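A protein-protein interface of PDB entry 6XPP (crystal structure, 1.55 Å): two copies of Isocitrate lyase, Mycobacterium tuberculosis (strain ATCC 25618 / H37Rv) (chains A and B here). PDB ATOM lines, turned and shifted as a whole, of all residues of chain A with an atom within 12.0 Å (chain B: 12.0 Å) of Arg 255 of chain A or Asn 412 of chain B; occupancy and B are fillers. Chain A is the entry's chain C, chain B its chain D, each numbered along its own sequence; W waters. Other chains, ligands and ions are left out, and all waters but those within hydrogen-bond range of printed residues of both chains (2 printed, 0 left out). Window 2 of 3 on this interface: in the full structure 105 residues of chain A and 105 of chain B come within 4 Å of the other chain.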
ATOM      1  N   LEU A 185      -1.159  13.390  22.262  1.00  0.00           N
ATOM      2  CA  LEU A 185      -2.545  13.711  21.833  1.00  0.00           C
ATOM      3  C   LEU A 185      -3.210  12.410  21.373  1.00  0.00           C
ATOM      4  O   LEU A 185      -2.671  11.787  20.457  1.00  0.00           O
ATOM      5  CB  LEU A 185      -2.477  14.731  20.696  1.00  0.00           C
ATOM      6  CG  LEU A 185      -3.817  15.113  20.069  1.00  0.00           C
ATOM      7  CD1 LEU A 185      -4.735  15.754  21.093  1.00  0.00           C
ATOM      8  CD2 LEU A 185      -3.589  16.047  18.878  1.00  0.00           C
ATOM      9  N   GLU A 188      -3.822  11.656  17.670  1.00  0.00           N
ATOM     10  CA  GLU A 188      -2.606  11.508  16.816  1.00  0.00           C
ATOM     11  C   GLU A 188      -1.628  10.529  17.480  1.00  0.00           C
ATOM     12  O   GLU A 188      -0.424  10.591  17.156  1.00  0.00           O
ATOM     13  CB  GLU A 188      -1.961  12.877  16.571  1.00  0.00           C
ATOM     14  CG  GLU A 188      -2.838  13.827  15.772  1.00  0.00           C
ATOM     15  CD  GLU A 188      -3.224  13.348  14.381  1.00  0.00           C
ATOM     16  OE1 GLU A 188      -2.483  12.517  13.823  1.00  0.00           O
ATOM     17  OE2 GLU A 188      -4.275  13.807  13.857  1.00  0.00           O
ATOM     18  N   LYS A 190       0.866   7.662  18.663  1.00  0.00           N
ATOM     19  CA  LYS A 190       1.826   6.811  17.921  1.00  0.00           C
ATOM     20  C   LYS A 190       2.584   5.891  18.885  1.00  0.00           C
ATOM     21  O   LYS A 190       2.840   6.283  20.042  1.00  0.00           O
ATOM     22  CB  LYS A 190       2.866   7.660  17.186  1.00  0.00           C
ATOM     23  CG  LYS A 190       2.326   8.678  16.197  1.00  0.00           C
ATOM     24  CD  LYS A 190       1.694   8.061  14.966  1.00  0.00           C
ATOM     25  CE  LYS A 190       1.428   9.080  13.876  1.00  0.00           C
ATOM     26  NZ  LYS A 190       0.614  10.224  14.352  1.00  0.00           N
ATOM     27  N   GLY A 196       5.672  11.419  13.740  1.00  0.00           N
ATOM     28  CA  GLY A 196       4.399  12.162  13.733  1.00  0.00           C
ATOM     29  C   GLY A 196       3.761  12.211  15.110  1.00  0.00           C
ATOM     30  O   GLY A 196       2.513  12.245  15.194  1.00  0.00           O
ATOM     31  N   VAL A 198       2.693  13.961  18.604  1.00  0.00           N
ATOM     32  CA  VAL A 198       2.249  15.287  19.101  1.00  0.00           C
ATOM     33  C   VAL A 198       2.107  15.170  20.619  1.00  0.00           C
ATOM     34  O   VAL A 198       1.293  14.345  21.084  1.00  0.00           O
ATOM     35  CB  VAL A 198       0.925  15.715  18.449  1.00  0.00           C
ATOM     36  CG1 VAL A 198       0.522  17.100  18.904  1.00  0.00           C
ATOM     37  CG2 VAL A 198       0.999  15.641  16.932  1.00  0.00           C
ATOM     38  N   THR A 235       8.316  16.330  17.914  1.00  0.00           N
ATOM     39  CA  THR A 235       8.690  17.720  17.523  1.00  0.00           C
ATOM     40  C   THR A 235       7.440  18.598  17.446  1.00  0.00           C
ATOM     41  O   THR A 235       7.559  19.752  16.969  1.00  0.00           O
ATOM     42  CB  THR A 235       9.487  17.737  16.214  1.00  0.00           C
ATOM     43  OG1 THR A 235       8.661  17.227  15.171  1.00  0.00           O
ATOM     44  CG2 THR A 235      10.758  16.916  16.303  1.00  0.00           C
ATOM     45  N   LEU A 236       6.286  18.095  17.903  1.00  0.00           N
ATOM     46  CA  LEU A 236       5.012  18.853  17.893  1.00  0.00           C
ATOM     47  C   LEU A 236       4.379  18.798  19.282  1.00  0.00           C
ATOM     48  O   LEU A 236       4.553  17.782  19.999  1.00  0.00           O
ATOM     49  CB  LEU A 236       4.063  18.272  16.845  1.00  0.00           C
ATOM     50  CG  LEU A 236       4.542  18.372  15.399  1.00  0.00           C
ATOM     51  CD1 LEU A 236       3.690  17.501  14.498  1.00  0.00           C
ATOM     52  CD2 LEU A 236       4.532  19.824  14.932  1.00  0.00           C
ATOM     53  N   ILE A 237       3.658  19.865  19.630  1.00  0.00           N
ATOM     54  CA  ILE A 237       2.844  19.938  20.873  1.00  0.00           C
ATOM     55  C   ILE A 237       1.556  20.692  20.538  1.00  0.00           C
ATOM     56  O   ILE A 237       1.564  21.559  19.638  1.00  0.00           O
ATOM     57  CB  ILE A 237       3.651  20.559  22.028  1.00  0.00           C
ATOM     58  CG1 ILE A 237       2.898  20.482  23.363  1.00  0.00           C
ATOM     59  CG2 ILE A 237       4.073  21.989  21.703  1.00  0.00           C
ATOM     60  CD1 ILE A 237       3.717  20.912  24.565  1.00  0.00           C
ATOM     61  N   THR A 238       0.447  20.338  21.180  1.00  0.00           N
ATOM     62  CA  THR A 238      -0.886  20.895  20.845  1.00  0.00           C
ATOM     63  C   THR A 238      -0.948  22.388  21.178  1.00  0.00           C
ATOM     64  O   THR A 238      -1.708  23.105  20.501  1.00  0.00           O
ATOM     65  CB  THR A 238      -2.007  20.144  21.572  1.00  0.00           C
ATOM     66  OG1 THR A 238      -1.734  20.194  22.971  1.00  0.00           O
ATOM     67  CG2 THR A 238      -2.136  18.714  21.109  1.00  0.00           C
ATOM     68  N   THR A 250       9.437  26.605  19.528  1.00  0.00           N
ATOM     69  CA  THR A 250      10.271  27.294  18.505  1.00  0.00           C
ATOM     70  C   THR A 250       9.438  27.636  17.264  1.00  0.00           C
ATOM     71  O   THR A 250       8.772  26.720  16.728  1.00  0.00           O
ATOM     72  CB  THR A 250      11.492  26.450  18.111  1.00  0.00           C
ATOM     73  OG1 THR A 250      12.181  27.132  17.063  1.00  0.00           O
ATOM     74  CG2 THR A 250      11.123  25.063  17.643  1.00  0.00           C
ATOM     75  N   ARG A 253       3.997  27.483  13.926  1.00  0.00           N
ATOM     76  CA  ARG A 253       2.876  26.508  14.028  1.00  0.00           C
ATOM     77  C   ARG A 253       2.693  25.807  12.677  1.00  0.00           C
ATOM     78  O   ARG A 253       2.972  26.442  11.629  1.00  0.00           O
ATOM     79  CB  ARG A 253       1.576  27.209  14.441  1.00  0.00           C
ATOM     80  CG  ARG A 253       1.535  27.643  15.900  1.00  0.00           C
ATOM     81  CD  ARG A 253       0.130  27.883  16.417  1.00  0.00           C
ATOM     82  NE  ARG A 253      -0.683  28.762  15.589  1.00  0.00           N
ATOM     83  CZ  ARG A 253      -1.856  29.285  15.945  1.00  0.00           C
ATOM     84  NH1 ARG A 253      -2.376  29.031  17.135  1.00  0.00           N
ATOM     85  NH2 ARG A 253      -2.509  30.071  15.101  1.00  0.00           N
ATOM     86  N   THR A 254       2.179  24.578  12.688  1.00  0.00           N
ATOM     87  CA  THR A 254       1.802  23.828  11.469  1.00  0.00           C
ATOM     88  C   THR A 254       0.436  24.329  10.990  1.00  0.00           C
ATOM     89  O   THR A 254      -0.232  25.057  11.748  1.00  0.00           O
ATOM     90  CB  THR A 254       1.756  22.312  11.710  1.00  0.00           C
ATOM     91  OG1 THR A 254       0.616  22.046  12.522  1.00  0.00           O
ATOM     92  CG2 THR A 254       2.983  21.751  12.381  1.00  0.00           C
ATOM     93  N   ARG A 255       0.043  23.931   9.784  1.00  0.00           N
ATOM     94  CA  ARG A 255      -1.282  24.213   9.173  1.00  0.00           C
ATOM     95  C   ARG A 255      -2.414  23.689  10.068  1.00  0.00           C
ATOM     96  O   ARG A 255      -3.504  24.252  10.013  1.00  0.00           O
ATOM     97  CB  ARG A 255      -1.353  23.553   7.790  1.00  0.00           C
ATOM     98  CG  ARG A 255      -1.032  22.061   7.807  1.00  0.00           C
ATOM     99  CD  ARG A 255      -0.680  21.503   6.447  1.00  0.00           C
ATOM    100  NE  ARG A 255      -1.918  21.380   5.703  1.00  0.00           N
ATOM    101  CZ  ARG A 255      -2.837  20.458   5.947  1.00  0.00           C
ATOM    102  NH1 ARG A 255      -3.945  20.423   5.230  1.00  0.00           N
ATOM    103  NH2 ARG A 255      -2.639  19.577   6.911  1.00  0.00           N
ATOM    104  N   GLU A 256      -2.155  22.624  10.841  1.00  0.00           N
ATOM    105  CA  GLU A 256      -3.159  22.011  11.754  1.00  0.00           C
ATOM    106  C   GLU A 256      -3.288  22.846  13.034  1.00  0.00           C
ATOM    107  O   GLU A 256      -4.260  22.624  13.767  1.00  0.00           O
ATOM    108  CB  GLU A 256      -2.783  20.565  12.118  1.00  0.00           C
ATOM    109  CG  GLU A 256      -2.714  19.652  10.909  1.00  0.00           C
ATOM    110  CD  GLU A 256      -1.306  19.339  10.417  1.00  0.00           C
ATOM    111  OE1 GLU A 256      -0.369  20.127  10.710  1.00  0.00           O
ATOM    112  OE2 GLU A 256      -1.153  18.284   9.769  1.00  0.00           O
ATOM    113  N   GLY A 257      -2.342  23.746  13.306  1.00  0.00           N
ATOM    114  CA  GLY A 257      -2.309  24.565  14.532  1.00  0.00           C
ATOM    115  C   GLY A 257      -1.453  23.945  15.628  1.00  0.00           C
ATOM    116  O   GLY A 257      -1.493  24.469  16.774  1.00  0.00           O
ATOM    117  N   PHE A 258      -0.670  22.908  15.323  1.00  0.00           N
ATOM    118  CA  PHE A 258       0.315  22.342  16.292  1.00  0.00           C
ATOM    119  C   PHE A 258       1.516  23.283  16.388  1.00  0.00           C
ATOM    120  O   PHE A 258       1.847  23.938  15.386  1.00  0.00           O
ATOM    121  CB  PHE A 258       0.776  20.932  15.907  1.00  0.00           C
ATOM    122  CG  PHE A 258      -0.336  19.925  15.755  1.00  0.00           C
ATOM    123  CD1 PHE A 258      -1.363  19.871  16.682  1.00  0.00           C
ATOM    124  CD2 PHE A 258      -0.375  19.051  14.677  1.00  0.00           C
ATOM    125  CE1 PHE A 258      -2.388  18.948  16.550  1.00  0.00           C
ATOM    126  CE2 PHE A 258      -1.417  18.151  14.533  1.00  0.00           C
ATOM    127  CZ  PHE A 258      -2.411  18.091  15.478  1.00  0.00           C
ATOM    128  N   TYR A 259       2.146  23.338  17.560  1.00  0.00           N
ATOM    129  CA  TYR A 259       3.386  24.108  17.811  1.00  0.00           C
ATOM    130  C   TYR A 259       4.594  23.193  17.637  1.00  0.00           C
ATOM    131  O   TYR A 259       4.605  22.052  18.141  1.00  0.00           O
ATOM    132  CB  TYR A 259       3.395  24.711  19.213  1.00  0.00           C
ATOM    133  CG  TYR A 259       2.385  25.801  19.439  1.00  0.00           C
ATOM    134  CD1 TYR A 259       1.049  25.500  19.617  1.00  0.00           C
ATOM    135  CD2 TYR A 259       2.766  27.134  19.487  1.00  0.00           C
ATOM    136  CE1 TYR A 259       0.105  26.491  19.828  1.00  0.00           C
ATOM    137  CE2 TYR A 259       1.836  28.137  19.702  1.00  0.00           C
ATOM    138  CZ  TYR A 259       0.501  27.815  19.874  1.00  0.00           C
ATOM    139  OH  TYR A 259      -0.427  28.794  20.079  1.00  0.00           O
ATOM    140  N   ARG A 260       5.610  23.684  16.929  1.00  0.00           N
ATOM    141  CA  ARG A 260       6.901  22.963  16.821  1.00  0.00           C
ATOM    142  C   ARG A 260       7.595  23.117  18.169  1.00  0.00           C
ATOM    143  O   ARG A 260       7.474  24.194  18.788  1.00  0.00           O
ATOM    144  CB  ARG A 260       7.723  23.469  15.636  1.00  0.00           C
ATOM    145  CG  ARG A 260       6.973  23.377  14.312  1.00  0.00           C
ATOM    146  CD  ARG A 260       7.805  23.773  13.102  1.00  0.00           C
ATOM    147  NE  ARG A 260       6.971  23.896  11.911  1.00  0.00           N
ATOM    148  CZ  ARG A 260       6.502  22.884  11.183  1.00  0.00           C
ATOM    149  NH1 ARG A 260       6.768  21.630  11.517  1.00  0.00           N
ATOM    150  NH2 ARG A 260       5.740  23.132  10.127  1.00  0.00           N
ATOM    151  N   PHE B 402      -1.965   2.749   6.489  1.00  0.00           N
ATOM    152  CA  PHE B 402      -2.690   3.843   7.176  1.00  0.00           C
ATOM    153  C   PHE B 402      -2.049   5.195   6.836  1.00  0.00           C
ATOM    154  O   PHE B 402      -2.791   6.174   6.734  1.00  0.00           O
ATOM    155  CB  PHE B 402      -2.834   3.540   8.670  1.00  0.00           C
ATOM    156  CG  PHE B 402      -3.990   2.602   8.914  1.00  0.00           C
ATOM    157  CD1 PHE B 402      -5.264   3.110   9.110  1.00  0.00           C
ATOM    158  CD2 PHE B 402      -3.827   1.227   8.834  1.00  0.00           C
ATOM    159  CE1 PHE B 402      -6.349   2.258   9.255  1.00  0.00           C
ATOM    160  CE2 PHE B 402      -4.914   0.378   8.993  1.00  0.00           C
ATOM    161  CZ  PHE B 402      -6.166   0.894   9.210  1.00  0.00           C
ATOM    162  N   ASP B 403      -0.730   5.256   6.641  1.00  0.00           N
ATOM    163  CA  ASP B 403      -0.085   6.488   6.123  1.00  0.00           C
ATOM    164  C   ASP B 403      -0.698   6.844   4.762  1.00  0.00           C
ATOM    165  O   ASP B 403      -0.967   8.027   4.534  1.00  0.00           O
ATOM    166  CB  ASP B 403       1.429   6.324   6.010  1.00  0.00           C
ATOM    167  CG  ASP B 403       2.170   6.595   7.303  1.00  0.00           C
ATOM    168  OD1 ASP B 403       1.505   6.920   8.322  1.00  0.00           O
ATOM    169  OD2 ASP B 403       3.417   6.486   7.278  1.00  0.00           O
ATOM    170  N   ARG B 404      -0.926   5.858   3.895  1.00  0.00           N
ATOM    171  CA  ARG B 404      -1.524   6.101   2.556  1.00  0.00           C
ATOM    172  C   ARG B 404      -2.969   6.599   2.715  1.00  0.00           C
ATOM    173  O   ARG B 404      -3.360   7.538   2.002  1.00  0.00           O
ATOM    174  CB  ARG B 404      -1.436   4.849   1.685  1.00  0.00           C
ATOM    175  CG  ARG B 404      -1.876   5.067   0.244  1.00  0.00           C
ATOM    176  CD  ARG B 404      -1.003   6.067  -0.500  1.00  0.00           C
ATOM    177  NE  ARG B 404      -1.256   5.981  -1.931  1.00  0.00           N
ATOM    178  CZ  ARG B 404      -0.676   5.120  -2.763  1.00  0.00           C
ATOM    179  NH1 ARG B 404       0.239   4.264  -2.331  1.00  0.00           N
ATOM    180  NH2 ARG B 404      -1.008   5.132  -4.041  1.00  0.00           N
ATOM    181  N   ILE B 405      -3.751   6.040   3.643  1.00  0.00           N
ATOM    182  CA  ILE B 405      -5.106   6.595   3.916  1.00  0.00           C
ATOM    183  C   ILE B 405      -4.948   8.050   4.364  1.00  0.00           C
ATOM    184  O   ILE B 405      -5.673   8.919   3.856  1.00  0.00           O
ATOM    185  CB  ILE B 405      -5.875   5.756   4.962  1.00  0.00           C
ATOM    186  CG1 ILE B 405      -6.142   4.339   4.461  1.00  0.00           C
ATOM    187  CG2 ILE B 405      -7.167   6.463   5.361  1.00  0.00           C
ATOM    188  CD1 ILE B 405      -6.824   3.457   5.481  1.00  0.00           C
ATOM    189  N   ALA B 406      -4.061   8.314   5.322  1.00  0.00           N
ATOM    190  CA  ALA B 406      -3.901   9.662   5.917  1.00  0.00           C
ATOM    191  C   ALA B 406      -3.544  10.670   4.820  1.00  0.00           C
ATOM    192  O   ALA B 406      -4.131  11.754   4.826  1.00  0.00           O
ATOM    193  CB  ALA B 406      -2.862   9.647   7.008  1.00  0.00           C
ATOM    194  N   THR B 407      -2.631  10.326   3.915  1.00  0.00           N
ATOM    195  CA  THR B 407      -2.165  11.266   2.853  1.00  0.00           C
ATOM    196  C   THR B 407      -3.203  11.341   1.731  1.00  0.00           C
ATOM    197  O   THR B 407      -3.199  12.344   1.013  1.00  0.00           O
ATOM    198  CB  THR B 407      -0.760  10.916   2.343  1.00  0.00           C
ATOM    199  OG1 THR B 407      -0.756   9.609   1.778  1.00  0.00           O
ATOM    200  CG2 THR B 407       0.289  10.997   3.426  1.00  0.00           C
ATOM    201  N   THR B 408      -4.083  10.346   1.587  1.00  0.00           N
ATOM    202  CA  THR B 408      -5.223  10.433   0.635  1.00  0.00           C
ATOM    203  C   THR B 408      -6.204  11.485   1.159  1.00  0.00           C
ATOM    204  O   THR B 408      -6.696  12.308   0.367  1.00  0.00           O
ATOM    205  CB  THR B 408      -5.887   9.073   0.412  1.00  0.00           C
ATOM    206  OG1 THR B 408      -4.890   8.165  -0.057  1.00  0.00           O
ATOM    207  CG2 THR B 408      -7.039   9.146  -0.563  1.00  0.00           C
ATOM    208  N   VAL B 409      -6.493  11.459   2.461  1.00  0.00           N
ATOM    209  CA  VAL B 409      -7.435  12.416   3.104  1.00  0.00           C
ATOM    210  C   VAL B 409      -6.786  13.806   3.127  1.00  0.00           C
ATOM    211  O   VAL B 409      -7.480  14.786   2.809  1.00  0.00           O
ATOM    212  CB  VAL B 409      -7.825  11.935   4.513  1.00  0.00           C
ATOM    213  CG1 VAL B 409      -8.610  12.998   5.264  1.00  0.00           C
ATOM    214  CG2 VAL B 409      -8.603  10.630   4.441  1.00  0.00           C
ATOM    215  N   ASP B 410      -5.505  13.884   3.498  1.00  0.00           N
ATOM    216  CA  ASP B 410      -4.772  15.167   3.667  1.00  0.00           C
ATOM    217  C   ASP B 410      -3.321  14.965   3.259  1.00  0.00           C
ATOM    218  O   ASP B 410      -2.496  14.563   4.080  1.00  0.00           O
ATOM    219  CB  ASP B 410      -4.860  15.679   5.103  1.00  0.00           C
ATOM    220  CG  ASP B 410      -4.137  17.000   5.325  1.00  0.00           C
ATOM    221  OD1 ASP B 410      -3.664  17.595   4.317  1.00  0.00           O
ATOM    222  OD2 ASP B 410      -4.044  17.410   6.517  1.00  0.00           O
ATOM    223  N   PRO B 411      -2.979  15.228   1.974  1.00  0.00           N
ATOM    224  CA  PRO B 411      -1.614  15.034   1.478  1.00  0.00           C
ATOM    225  C   PRO B 411      -0.549  15.743   2.321  1.00  0.00           C
ATOM    226  O   PRO B 411       0.587  15.292   2.331  1.00  0.00           O
ATOM    227  CB  PRO B 411      -1.648  15.647   0.064  1.00  0.00           C
ATOM    228  CG  PRO B 411      -3.098  15.561  -0.361  1.00  0.00           C
ATOM    229  CD  PRO B 411      -3.900  15.692   0.919  1.00  0.00           C
ATOM    230  N   ASN B 412      -0.938  16.832   2.998  1.00  0.00           N
ATOM    231  CA  ASN B 412      -0.009  17.761   3.689  1.00  0.00           C
ATOM    232  C   ASN B 412       0.013  17.471   5.195  1.00  0.00           C
ATOM    233  O   ASN B 412       0.590  18.281   5.942  1.00  0.00           O
ATOM    234  CB  ASN B 412      -0.380  19.207   3.361  1.00  0.00           C
ATOM    235  CG  ASN B 412      -0.306  19.458   1.865  1.00  0.00           C
ATOM    236  OD1 ASN B 412       0.514  18.840   1.183  1.00  0.00           O
ATOM    237  ND2 ASN B 412      -1.180  20.303   1.346  1.00  0.00           N
ATOM    238  N   SER B 413      -0.551  16.343   5.630  1.00  0.00           N
ATOM    239  CA  SER B 413      -0.577  15.952   7.062  1.00  0.00           C
ATOM    240  C   SER B 413       0.827  16.028   7.674  1.00  0.00           C
ATOM    241  O   SER B 413       1.764  15.491   7.071  1.00  0.00           O
ATOM    242  CB  SER B 413      -1.166  14.588   7.245  1.00  0.00           C
ATOM    243  OG  SER B 413      -1.033  14.197   8.598  1.00  0.00           O
ATOM    244  N   SER B 414       0.942  16.636   8.857  1.00  0.00           N
ATOM    245  CA  SER B 414       2.186  16.731   9.667  1.00  0.00           C
ATOM    246  C   SER B 414       2.369  15.496  10.571  1.00  0.00           C
ATOM    247  O   SER B 414       3.408  15.436  11.249  1.00  0.00           O
ATOM    248  CB  SER B 414       2.190  17.989  10.510  1.00  0.00           C
ATOM    249  OG  SER B 414       2.013  19.151   9.713  1.00  0.00           O
ATOM    250  N   THR B 415       1.415  14.555  10.603  1.00  0.00           N
ATOM    251  CA  THR B 415       1.338  13.520  11.675  1.00  0.00           C
ATOM    252  C   THR B 415       1.276  12.099  11.100  1.00  0.00           C
ATOM    253  O   THR B 415       0.706  11.218  11.780  1.00  0.00           O
ATOM    254  CB  THR B 415       0.151  13.810  12.603  1.00  0.00           C
ATOM    255  OG1 THR B 415      -1.061  13.791  11.852  1.00  0.00           O
ATOM    256  CG2 THR B 415       0.264  15.149  13.296  1.00  0.00           C
ATOM    257  N   THR B 416       1.888  11.840   9.941  1.00  0.00           N
ATOM    258  CA  THR B 416       2.022  10.459   9.390  1.00  0.00           C
ATOM    259  C   THR B 416       3.106   9.720  10.195  1.00  0.00           C
ATOM    260  O   THR B 416       3.913  10.397  10.888  1.00  0.00           O
ATOM    261  CB  THR B 416       2.255  10.481   7.873  1.00  0.00           C
ATOM    262  OG1 THR B 416       3.517  11.101   7.619  1.00  0.00           O
ATOM    263  CG2 THR B 416       1.152  11.226   7.151  1.00  0.00           C
ATOM    264  N   ALA B 417       3.122   8.391  10.117  1.00  0.00           N
ATOM    265  CA  ALA B 417       3.782   7.492  11.096  1.00  0.00           C
ATOM    266  C   ALA B 417       5.174   7.025  10.643  1.00  0.00           C
ATOM    267  O   ALA B 417       6.075   6.992  11.496  1.00  0.00           O
ATOM    268  CB  ALA B 417       2.885   6.310  11.372  1.00  0.00           C
ATOM    269  N   THR B 419       7.519   8.131   8.375  1.00  0.00           N
ATOM    270  CA  THR B 419       8.554   9.195   8.269  1.00  0.00           C
ATOM    271  C   THR B 419       9.019   9.560   9.683  1.00  0.00           C
ATOM    272  O   THR B 419       8.171   9.973  10.501  1.00  0.00           O
ATOM    273  CB  THR B 419       8.050  10.406   7.475  1.00  0.00           C
ATOM    274  OG1 THR B 419       7.780   9.940   6.155  1.00  0.00           O
ATOM    275  CG2 THR B 419       9.043  11.548   7.415  1.00  0.00           C
HETATM  276  O   HOH W   1      -2.402  16.118  10.809  1.00  0.00           O
HETATM  277  O   HOH W   2      -2.835  21.781   2.895  1.00  0.00           O
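The guanidinium group (NH2) of Arg 255 of chain A is in salt-bridge range of the side-chain carboxylate (OE2) of Glu 256 of chain A (3.5 Å).
The side-chain carboxylate (OD1) of Asp 410 of chain B lies close to the backbone NH (N) of Asn 412 of chain B (3.1 Å).
The backbone NH (N) of Leu 185 of chain A sits at hydrogen-bond distance from the backbone carbonyl oxygen (O) of Val 198 of chain A, 2.9 Å away.
The side-chain carboxylate (OD1) of Asp 403 of chain B sits at hydrogen-bond distance from the backbone NH (N) of Ala 417 of chain B (2.8 Å).
The side-chain hydroxyl (OG1) of Thr 254 of chain A lies within hydrogen-bond range of the backbone NH (N) of Phe 258 of chain A, at 3.2 Å.
NZ of Lys 190 of chain A sits at hydrogen-bond distance from O of Gly 196 of chain A (2.9 Å).
Printed residues of chain B within 4 Å of Arg 255 of chain A: Asp 410 and Asn 412.
Printed residues of chain A within 4 Å of Asn 412 of chain B: Arg 255 (3.5 Å).
Of chain B, only Ser 414 (3.7 Å) comes within 4 Å of Thr 254 of chain A.
No residue of chain B comes within 4 Å of Gly 257 of chain A.
No residue of chain A comes within 4 Å of Pro 411 of chain B.
Ser 413 of chain B touches just one residue of chain A: Glu 256 (3.6 Å).
Printed residues of chain A within 4 Å of Thr 415 of chain B: Glu 188, Lys 190, Gly 196, Val 198 and Phe 258.
Of the printed residues of chain B, Glu 188 of chain A touches Thr 415.
Of the printed residues of chain A, Thr 416 of chain B touches Gly 196 (3.4 Å).
Printed residues of chain A within 4 Å of Asp 410 of chain B: Arg 255.
Thr 419 of chain B touches none of the printed residues of chain A.
Arg 260 of chain A touches none of the printed residues of chain B.
The nearest printed residue of chain A that does not touch Asn 412 of chain B is Glu 256 of chain A (4.2 Å).
NZ of Lys 190 of chain A lies within hydrogen-bond range of O of Thr 415 of chain B (2.8 Å).
The side-chain carboxylate (OE1) of Glu 188 of chain A lies within hydrogen-bond range of the side-chain hydroxyl (OG1) of Thr 415 of chain B (2.7 Å).
OE1 of Glu 256 of chain A sits at hydrogen-bond distance from OG of Ser 414 of chain B.
The side-chain carboxylate (OD2) of Asp 410 of chain B lies within salt-bridge range of the guanidinium group (NH2) of Arg 255 of chain A, 2.6 Å away.
No position is printed for both chains.
Of the 13 pairs that touch across the chains among the printed residues, none has its exchanged pair printed and touching as well.
Of the 17 printed residues of chain B, 7 touch a printed residue of chain A.
Printed residues of chain B that touch a printed residue of chain A: Asp 410, Asn 412, Ser 413, Ser 414, Thr 415, Thr 416 and Ala 417.
Hydrophobic or aromatic side chains of chain A that line the printed part of chain B: Val 198, Leu 236 and Phe 258.
Among the printed residues, 13 pairs touch across the chains.
CE of Lys 190 of chain A touches CA of Ala 417 of chain B, at 3.97 Å.
Thr 415 of chain B touches Gly 196 of chain A.
O of Thr 416 of chain B touches CA of Gly 196 of chain A, at 3.4 Å.
CG2 of Thr 415 of chain B touches CG2 of Val 198 of chain A, at 3.7 Å.
Leu 236 of chain A touches Ser 414 of chain B (CD1 to O, 3.9 Å).
Ser 414 of chain B touches Thr 254 of chain A.
Arg 255 of chain A touches Asn 412 of chain B.
CA of Ser 413 of chain B touches OE2 of Glu 256 of chain A, 3.6 Å away.
Thr 415 of chain B touches Phe 258 of chain A.
Water W2 lies within hydrogen-bond range of the side-chain amide nitrogen (ND2) of Asn 412 of chain B and the guanidinium group (NH1) of Arg 255 of chain A.
Water W1 lies within hydrogen-bond range of the side-chain carboxylate of Glu 256 of chain A, the side-chain hydroxyl of Thr 415 of chain B and the side-chain hydroxyl of Ser 413 of chain B.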
